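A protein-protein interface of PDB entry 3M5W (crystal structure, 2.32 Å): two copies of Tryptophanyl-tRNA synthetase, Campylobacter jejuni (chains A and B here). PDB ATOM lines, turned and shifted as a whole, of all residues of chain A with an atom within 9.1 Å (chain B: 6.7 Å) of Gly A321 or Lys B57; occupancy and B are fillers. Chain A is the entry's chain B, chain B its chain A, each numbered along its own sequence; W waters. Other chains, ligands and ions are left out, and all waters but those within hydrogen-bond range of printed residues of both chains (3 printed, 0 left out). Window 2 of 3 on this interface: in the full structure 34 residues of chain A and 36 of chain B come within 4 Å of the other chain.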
ATOM      1  N   ILE A  94      13.393   9.337  -3.760  1.00  0.00           N
ATOM      2  CA  ILE A  94      12.061   9.269  -4.350  1.00  0.00           C
ATOM      3  C   ILE A  94      12.021   9.549  -5.866  1.00  0.00           C
ATOM      4  O   ILE A  94      11.335   8.849  -6.609  1.00  0.00           O
ATOM      5  CB  ILE A  94      11.151  10.205  -3.600  1.00  0.00           C
ATOM      6  CG1 ILE A  94      10.845   9.571  -2.258  1.00  0.00           C
ATOM      7  CG2 ILE A  94       9.874  10.441  -4.345  1.00  0.00           C
ATOM      8  CD1 ILE A  94      10.798  10.577  -1.127  1.00  0.00           C
ATOM      9  N   TRP A 167       0.907  11.368  -9.558  1.00  0.00           N
ATOM     10  CA  TRP A 167       0.423  11.735  -8.227  1.00  0.00           C
ATOM     11  C   TRP A 167      -0.396  13.019  -8.161  1.00  0.00           C
ATOM     12  O   TRP A 167      -0.880  13.419  -7.074  1.00  0.00           O
ATOM     13  CB  TRP A 167       1.614  11.930  -7.311  1.00  0.00           C
ATOM     14  CG  TRP A 167       2.214  10.707  -6.738  1.00  0.00           C
ATOM     15  CD1 TRP A 167       1.701   9.411  -6.748  1.00  0.00           C
ATOM     16  CD2 TRP A 167       3.448  10.643  -6.031  1.00  0.00           C
ATOM     17  NE1 TRP A 167       2.557   8.565  -6.090  1.00  0.00           N
ATOM     18  CE2 TRP A 167       3.643   9.290  -5.647  1.00  0.00           C
ATOM     19  CE3 TRP A 167       4.429  11.605  -5.693  1.00  0.00           C
ATOM     20  CZ2 TRP A 167       4.768   8.875  -4.930  1.00  0.00           C
ATOM     21  CZ3 TRP A 167       5.552  11.195  -4.982  1.00  0.00           C
ATOM     22  CH2 TRP A 167       5.708   9.833  -4.603  1.00  0.00           C
ATOM     23  N   MET A 313       7.931  18.156   1.541  1.00  0.00           N
ATOM     24  CA  MET A 313       8.040  16.743   1.911  1.00  0.00           C
ATOM     25  C   MET A 313       6.780  16.223   2.556  1.00  0.00           C
ATOM     26  O   MET A 313       6.483  15.052   2.437  1.00  0.00           O
ATOM     27  CB  MET A 313       9.227  16.495   2.855  1.00  0.00           C
ATOM     28  CG  MET A 313      10.575  16.660   2.185  1.00  0.00           C
ATOM     29  SD  MET A 313      10.786  15.758   0.440  1.00  0.00           S
ATOM     30  CE  MET A 313      11.050  13.893   1.081  1.00  0.00           C
ATOM     31  N   GLN A 314       6.034  17.077   3.256  1.00  0.00           N
ATOM     32  CA  GLN A 314       4.735  16.633   3.802  1.00  0.00           C
ATOM     33  C   GLN A 314       3.806  16.151   2.696  1.00  0.00           C
ATOM     34  O   GLN A 314       3.202  15.076   2.788  1.00  0.00           O
ATOM     35  CB  GLN A 314       4.032  17.748   4.573  1.00  0.00           C
ATOM     36  CG  GLN A 314       4.275  17.770   6.070  1.00  0.00           C
ATOM     37  CD  GLN A 314       3.580  18.983   6.756  1.00  0.00           C
ATOM     38  OE1 GLN A 314       3.034  19.867   6.088  1.00  0.00           O
ATOM     39  NE2 GLN A 314       3.612  19.016   8.088  1.00  0.00           N
ATOM     40  N   LYS A 315       3.684  16.932   1.641  1.00  0.00           N
ATOM     41  CA  LYS A 315       2.913  16.494   0.500  1.00  0.00           C
ATOM     42  C   LYS A 315       3.443  15.150   0.041  1.00  0.00           C
ATOM     43  O   LYS A 315       2.718  14.176  -0.001  1.00  0.00           O
ATOM     44  CB  LYS A 315       3.013  17.501  -0.634  1.00  0.00           C
ATOM     45  CG  LYS A 315       1.774  18.313  -0.833  1.00  0.00           C
ATOM     46  CD  LYS A 315       1.518  19.210   0.348  1.00  0.00           C
ATOM     47  CE  LYS A 315       0.237  20.000   0.166  1.00  0.00           C
ATOM     48  NZ  LYS A 315      -0.827  19.204  -0.510  1.00  0.00           N
ATOM     49  N   ILE A 316       4.719  15.109  -0.306  1.00  0.00           N
ATOM     50  CA  ILE A 316       5.348  13.855  -0.770  1.00  0.00           C
ATOM     51  C   ILE A 316       5.137  12.569   0.087  1.00  0.00           C
ATOM     52  O   ILE A 316       4.843  11.501  -0.439  1.00  0.00           O
ATOM     53  CB  ILE A 316       6.863  14.061  -0.884  1.00  0.00           C
ATOM     54  CG1 ILE A 316       7.181  15.256  -1.800  1.00  0.00           C
ATOM     55  CG2 ILE A 316       7.543  12.765  -1.309  1.00  0.00           C
ATOM     56  CD1 ILE A 316       7.009  14.980  -3.274  1.00  0.00           C
ATOM     57  N   TYR A 317       5.375  12.698   1.391  1.00  0.00           N
ATOM     58  CA  TYR A 317       5.066  11.709   2.397  1.00  0.00           C
ATOM     59  C   TYR A 317       3.650  11.167   2.335  1.00  0.00           C
ATOM     60  O   TYR A 317       3.447   9.976   2.509  1.00  0.00           O
ATOM     61  CB  TYR A 317       5.251  12.318   3.777  1.00  0.00           C
ATOM     62  CG  TYR A 317       6.698  12.351   4.204  1.00  0.00           C
ATOM     63  CD1 TYR A 317       7.722  12.169   3.288  1.00  0.00           C
ATOM     64  CD2 TYR A 317       7.038  12.590   5.521  1.00  0.00           C
ATOM     65  CE1 TYR A 317       9.075  12.208   3.688  1.00  0.00           C
ATOM     66  CE2 TYR A 317       8.357  12.634   5.929  1.00  0.00           C
ATOM     67  CZ  TYR A 317       9.376  12.455   5.014  1.00  0.00           C
ATOM     68  OH  TYR A 317      10.692  12.522   5.467  1.00  0.00           O
ATOM     69  N   GLU A 318       2.667  12.035   2.146  1.00  0.00           N
ATOM     70  CA  GLU A 318       1.314  11.556   1.894  1.00  0.00           C
ATOM     71  C   GLU A 318       1.289  10.557   0.745  1.00  0.00           C
ATOM     72  O   GLU A 318       0.665   9.506   0.878  1.00  0.00           O
ATOM     73  CB  GLU A 318       0.352  12.691   1.559  1.00  0.00           C
ATOM     74  CG  GLU A 318      -0.208  13.389   2.763  1.00  0.00           C
ATOM     75  CD  GLU A 318      -1.080  14.585   2.386  1.00  0.00           C
ATOM     76  OE1 GLU A 318      -1.313  14.805   1.169  1.00  0.00           O
ATOM     77  OE2 GLU A 318      -1.524  15.312   3.310  1.00  0.00           O
ATOM     78  N   LYS A 319       1.988  10.872  -0.354  1.00  0.00           N
ATOM     79  CA  LYS A 319       1.834  10.148  -1.618  1.00  0.00           C
ATOM     80  C   LYS A 319       2.704   8.907  -1.679  1.00  0.00           C
ATOM     81  O   LYS A 319       2.452   7.998  -2.451  1.00  0.00           O
ATOM     82  CB  LYS A 319       2.067  11.078  -2.824  1.00  0.00           C
ATOM     83  CG  LYS A 319       0.994  12.199  -2.950  1.00  0.00           C
ATOM     84  CD  LYS A 319      -0.097  11.718  -3.907  1.00  0.00           C
ATOM     85  CE  LYS A 319      -1.104  12.768  -4.268  1.00  0.00           C
ATOM     86  NZ  LYS A 319      -2.376  12.656  -3.481  1.00  0.00           N
ATOM     87  N   ILE A 320       3.710   8.834  -0.829  1.00  0.00           N
ATOM     88  CA  ILE A 320       4.614   7.693  -0.865  1.00  0.00           C
ATOM     89  C   ILE A 320       4.386   6.831   0.367  1.00  0.00           C
ATOM     90  O   ILE A 320       5.015   5.796   0.524  1.00  0.00           O
ATOM     91  CB  ILE A 320       6.093   8.152  -0.887  1.00  0.00           C
ATOM     92  CG1 ILE A 320       7.018   6.991  -1.244  1.00  0.00           C
ATOM     93  CG2 ILE A 320       6.493   8.748   0.465  1.00  0.00           C
ATOM     94  CD1 ILE A 320       6.958   6.646  -2.705  1.00  0.00           C
ATOM     95  N   GLY A 321       3.516   7.288   1.263  1.00  0.00           N
ATOM     96  CA  GLY A 321       3.225   6.550   2.470  1.00  0.00           C
ATOM     97  C   GLY A 321       4.166   6.692   3.671  1.00  0.00           C
ATOM     98  O   GLY A 321       4.131   5.849   4.536  1.00  0.00           O
ATOM     99  N   LEU A 322       4.965   7.746   3.733  1.00  0.00           N
ATOM    100  CA  LEU A 322       5.788   7.971   4.906  1.00  0.00           C
ATOM    101  C   LEU A 322       5.010   8.780   5.922  1.00  0.00           C
ATOM    102  O   LEU A 322       4.079   9.495   5.572  1.00  0.00           O
ATOM    103  CB  LEU A 322       7.081   8.694   4.548  1.00  0.00           C
ATOM    104  CG  LEU A 322       8.148   7.860   3.851  1.00  0.00           C
ATOM    105  CD1 LEU A 322       9.474   8.559   3.896  1.00  0.00           C
ATOM    106  CD2 LEU A 322       8.246   6.497   4.482  1.00  0.00           C
ATOM    107  N   ASN B  43      11.789  -0.241   3.961  1.00  0.00           N
ATOM    108  CA  ASN B  43      10.658   0.339   3.249  1.00  0.00           C
ATOM    109  C   ASN B  43      11.097   1.344   2.190  1.00  0.00           C
ATOM    110  O   ASN B  43      10.304   1.756   1.342  1.00  0.00           O
ATOM    111  CB  ASN B  43       9.689   1.003   4.231  1.00  0.00           C
ATOM    112  CG  ASN B  43      10.334   2.129   5.014  1.00  0.00           C
ATOM    113  OD1 ASN B  43      11.499   2.044   5.402  1.00  0.00           O
ATOM    114  ND2 ASN B  43       9.576   3.195   5.251  1.00  0.00           N
ATOM    115  N   MET B  47      10.160   1.124  -2.415  1.00  0.00           N
ATOM    116  CA  MET B  47       9.673   2.189  -3.297  1.00  0.00           C
ATOM    117  C   MET B  47      10.184   2.039  -4.720  1.00  0.00           C
ATOM    118  O   MET B  47       9.666   2.676  -5.646  1.00  0.00           O
ATOM    119  CB  MET B  47      10.060   3.560  -2.790  1.00  0.00           C
ATOM    120  CG  MET B  47       9.480   3.973  -1.467  1.00  0.00           C
ATOM    121  SD  MET B  47      10.481   5.595  -0.725  1.00  0.00           S
ATOM    122  CE  MET B  47       9.800   5.392   1.141  1.00  0.00           C
ATOM    123  N   GLN B  51       4.870   2.994  -6.067  1.00  0.00           N
ATOM    124  CA  GLN B  51       4.687   4.327  -5.548  1.00  0.00           C
ATOM    125  C   GLN B  51       3.282   4.606  -5.068  1.00  0.00           C
ATOM    126  O   GLN B  51       2.914   5.754  -4.856  1.00  0.00           O
ATOM    127  CB  GLN B  51       5.205   5.390  -6.530  1.00  0.00           C
ATOM    128  CG  GLN B  51       6.728   5.229  -6.811  1.00  0.00           C
ATOM    129  CD  GLN B  51       7.025   4.157  -7.875  1.00  0.00           C
ATOM    130  OE1 GLN B  51       6.326   4.074  -8.883  1.00  0.00           O
ATOM    131  NE2 GLN B  51       8.050   3.328  -7.641  1.00  0.00           N
ATOM    132  N   ASP B  52       2.499   3.543  -4.874  1.00  0.00           N
ATOM    133  CA  ASP B  52       1.219   3.644  -4.186  1.00  0.00           C
ATOM    134  C   ASP B  52       1.440   3.768  -2.673  1.00  0.00           C
ATOM    135  O   ASP B  52       1.688   2.793  -1.960  1.00  0.00           O
ATOM    136  CB  ASP B  52       0.348   2.442  -4.517  1.00  0.00           C
ATOM    137  CG  ASP B  52      -0.942   2.410  -3.713  1.00  0.00           C
ATOM    138  OD1 ASP B  52      -1.319   3.439  -3.104  1.00  0.00           O
ATOM    139  OD2 ASP B  52      -1.586   1.346  -3.707  1.00  0.00           O
ATOM    140  N   GLY B  53       1.354   4.993  -2.182  1.00  0.00           N
ATOM    141  CA  GLY B  53       1.716   5.296  -0.810  1.00  0.00           C
ATOM    142  C   GLY B  53       0.920   4.525   0.221  1.00  0.00           C
ATOM    143  O   GLY B  53       1.473   3.944   1.176  1.00  0.00           O
ATOM    144  N   GLU B  54      -0.387   4.527   0.043  1.00  0.00           N
ATOM    145  CA  GLU B  54      -1.268   3.955   1.053  1.00  0.00           C
ATOM    146  C   GLU B  54      -1.035   2.468   1.180  1.00  0.00           C
ATOM    147  O   GLU B  54      -1.091   1.932   2.265  1.00  0.00           O
ATOM    148  CB  GLU B  54      -2.734   4.271   0.767  1.00  0.00           C
ATOM    149  CG  GLU B  54      -3.168   5.599   1.336  1.00  0.00           C
ATOM    150  CD  GLU B  54      -4.503   6.070   0.768  1.00  0.00           C
ATOM    151  OE1 GLU B  54      -5.222   5.247   0.149  1.00  0.00           O
ATOM    152  OE2 GLU B  54      -4.835   7.270   0.936  1.00  0.00           O
ATOM    153  N   LYS B  55      -0.718   1.827   0.065  1.00  0.00           N
ATOM    154  CA  LYS B  55      -0.390   0.401   0.059  1.00  0.00           C
ATOM    155  C   LYS B  55       0.973   0.161   0.670  1.00  0.00           C
ATOM    156  O   LYS B  55       1.174  -0.807   1.418  1.00  0.00           O
ATOM    157  CB  LYS B  55      -0.441  -0.157  -1.368  1.00  0.00           C
ATOM    158  CG  LYS B  55       0.211  -1.514  -1.553  1.00  0.00           C
ATOM    159  CD  LYS B  55      -0.223  -2.178  -2.870  1.00  0.00           C
ATOM    160  CE  LYS B  55       0.267  -1.420  -4.118  1.00  0.00           C
ATOM    161  NZ  LYS B  55       1.751  -1.496  -4.331  1.00  0.00           N
ATOM    162  N   LEU B  56       1.912   1.053   0.362  1.00  0.00           N
ATOM    163  CA  LEU B  56       3.250   0.953   0.941  1.00  0.00           C
ATOM    164  C   LEU B  56       3.198   1.160   2.450  1.00  0.00           C
ATOM    165  O   LEU B  56       3.909   0.512   3.175  1.00  0.00           O
ATOM    166  CB  LEU B  56       4.237   1.966   0.308  1.00  0.00           C
ATOM    167  CG  LEU B  56       4.614   1.822  -1.169  1.00  0.00           C
ATOM    168  CD1 LEU B  56       5.291   3.091  -1.617  1.00  0.00           C
ATOM    169  CD2 LEU B  56       5.504   0.630  -1.423  1.00  0.00           C
ATOM    170  N   LYS B  57       2.380   2.091   2.913  1.00  0.00           N
ATOM    171  CA  LYS B  57       2.330   2.419   4.325  1.00  0.00           C
ATOM    172  C   LYS B  57       1.854   1.209   5.116  1.00  0.00           C
ATOM    173  O   LYS B  57       2.511   0.756   6.075  1.00  0.00           O
ATOM    174  CB  LYS B  57       1.353   3.561   4.540  1.00  0.00           C
ATOM    175  CG  LYS B  57       1.501   4.334   5.861  1.00  0.00           C
ATOM    176  CD  LYS B  57       0.381   5.381   5.983  1.00  0.00           C
ATOM    177  CE  LYS B  57       0.382   6.148   7.323  1.00  0.00           C
ATOM    178  NZ  LYS B  57       1.205   7.403   7.311  1.00  0.00           N
ATOM    179  N   GLN B  58       0.710   0.676   4.680  1.00  0.00           N
ATOM    180  CA  GLN B  58       0.111  -0.486   5.297  1.00  0.00           C
ATOM    181  C   GLN B  58       1.059  -1.681   5.310  1.00  0.00           C
ATOM    182  O   GLN B  58       1.175  -2.390   6.307  1.00  0.00           O
ATOM    183  CB  GLN B  58      -1.200  -0.829   4.564  1.00  0.00           C
ATOM    184  CG  GLN B  58      -2.367  -0.980   5.502  1.00  0.00           C
ATOM    185  CD  GLN B  58      -2.274  -0.040   6.710  1.00  0.00           C
ATOM    186  OE1 GLN B  58      -1.956   1.152   6.582  1.00  0.00           O
ATOM    187  NE2 GLN B  58      -2.559  -0.579   7.888  1.00  0.00           N
ATOM    188  N   ASN B  59       1.735  -1.899   4.188  1.00  0.00           N
ATOM    189  CA  ASN B  59       2.657  -3.004   4.061  1.00  0.00           C
ATOM    190  C   ASN B  59       3.713  -2.937   5.134  1.00  0.00           C
ATOM    191  O   ASN B  59       4.132  -3.961   5.662  1.00  0.00           O
ATOM    192  CB  ASN B  59       3.340  -2.964   2.708  1.00  0.00           C
ATOM    193  CG  ASN B  59       2.501  -3.554   1.643  1.00  0.00           C
ATOM    194  OD1 ASN B  59       2.920  -3.634   0.498  1.00  0.00           O
ATOM    195  ND2 ASN B  59       1.287  -3.977   2.007  1.00  0.00           N
ATOM    196  N   SER B  60       4.119  -1.719   5.470  1.00  0.00           N
ATOM    197  CA  SER B  60       5.090  -1.524   6.540  1.00  0.00           C
ATOM    198  C   SER B  60       4.547  -1.778   7.963  1.00  0.00           C
ATOM    199  O   SER B  60       5.189  -2.440   8.761  1.00  0.00           O
ATOM    200  CB  SER B  60       5.729  -0.120   6.404  1.00  0.00           C
ATOM    201  OG  SER B  60       6.503  -0.072   5.220  1.00  0.00           O
ATOM    202  N   LEU B  61       3.380  -1.242   8.290  1.00  0.00           N
ATOM    203  CA  LEU B  61       2.758  -1.550   9.552  1.00  0.00           C
ATOM    204  C   LEU B  61       2.567  -3.042   9.665  1.00  0.00           C
ATOM    205  O   LEU B  61       2.801  -3.609  10.726  1.00  0.00           O
ATOM    206  CB  LEU B  61       1.399  -0.892   9.646  1.00  0.00           C
ATOM    207  CG  LEU B  61       1.518   0.571  10.025  1.00  0.00           C
ATOM    208  CD1 LEU B  61       0.191   0.959  10.617  1.00  0.00           C
ATOM    209  CD2 LEU B  61       2.744   0.832  11.045  1.00  0.00           C
ATOM    210  N   LYS B  62       2.127  -3.671   8.572  1.00  0.00           N
ATOM    211  CA  LYS B  62       1.747  -5.072   8.640  1.00  0.00           C
ATOM    212  C   LYS B  62       3.008  -5.919   8.779  1.00  0.00           C
ATOM    213  O   LYS B  62       3.023  -6.884   9.523  1.00  0.00           O
ATOM    214  CB  LYS B  62       0.935  -5.467   7.411  1.00  0.00           C
ATOM    215  CG  LYS B  62      -0.512  -5.033   7.458  1.00  0.00           C
ATOM    216  CD  LYS B  62      -1.183  -5.338   6.138  1.00  0.00           C
ATOM    217  CE  LYS B  62      -0.590  -6.631   5.545  1.00  0.00           C
ATOM    218  NZ  LYS B  62      -1.058  -6.994   4.163  1.00  0.00           N
HETATM  219  O   HOH W   1       0.821   8.479   4.126  1.00  0.00           O
HETATM  220  O   HOH W   2       0.011   7.429  -3.589  1.00  0.00           O
HETATM  221  O   HOH W   3       0.033   6.425  -6.522  1.00  0.00           O
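No position is printed for both chains.
The backbone carbonyl oxygen (O) of Met B47 is in hydrogen-bond range of the side-chain amide nitrogen (NE2) of Gln B51, at 2.6 Å.
The side-chain hydroxyl (OG) of Ser B60 lies within hydrogen-bond range of the backbone carbonyl oxygen (O) of Leu B56 (3.4 Å).
The backbone carbonyl oxygen (O) of Tyr A317 is in hydrogen-bond range of the backbone NH (N) of Leu A322, 3.0 Å away.
The backbone carbonyl oxygen (O) of Gln B51 lies within hydrogen-bond range of the indole nitrogen (NE1) of Trp A167, 3.1 Å away.
The backbone NH of Gly B53 lies within hydrogen-bond range of the backbone carbonyl oxygen of Lys A319 (3.2 Å).
The backbone carbonyl oxygen of Gln B51 lies close to the backbone carbonyl oxygen of Lys A319.
Water W2 bridges O of Lys A319 (2.8 Å) and N of Gly B53 (3.1 Å).
Water W3 bridges NE1 of Trp A167 (3.3 Å) and O of Gln B51 (3.4 Å).
Water W1 lies within hydrogen-bond range of NZ of Lys B57 (3.4 Å), O of Glu A318 (3.4 Å) and O of Tyr A317 (3.4 Å).
Of the printed residues of chain B, Trp A167 touches Gln B51.
Printed residues of chain B within 4 Å of Lys A319: Gln B51 and Gly B53.
Gly A321 touches just these residues of chain B: Gly B53 (3.4 Å) and Lys B57 (3.3 Å).
Of the printed residues of chain B, Leu A322 touches Asn B43 (3.6 Å), Met B47 (3.8 Å) and Lys B57 (3.96 Å).
Of chain A, only Gly A321 (3.3 Å) and Leu A322 (3.96 Å) come within 4 Å of Lys B57.
Ser B60 touches none of the printed residues of chain A.
Leu B61 touches none of the printed residues of chain A.
The nearest printed residue of chain A that does not touch Met B47 is Ile A94 (4.3 Å).
Of the 14 printed residues of chain B, 6 touch a printed residue of chain A.
Printed residues of chain B that touch a printed residue of chain A: Asn B43, Met B47, Gln B51, Gly B53, Leu B56 and Lys B57.
Hydrophobic or aromatic side chains of chain B that line the printed part of chain A: Met B47 and Leu B56.
Among the printed residues, no Asp or Glu carboxylate lies within 4 Å of a Lys or Arg side-chain nitrogen of the other chain.
Among the printed residues, pairs that only touch across the chains: Ile A320 with Gly B53 (3.3 Å), Gly A321 with Lys B57 (3.3 Å), Gly A321 with Gly B53 (3.4 Å), Ile A320 with Leu B56 (3.5 Å), Leu A322 with Asn B43 (3.6 Å), Ile A320 with Met B47 (3.8 Å), Leu A322 with Met B47 (3.8 Å) and Leu A322 with Lys B57 (3.96 Å).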
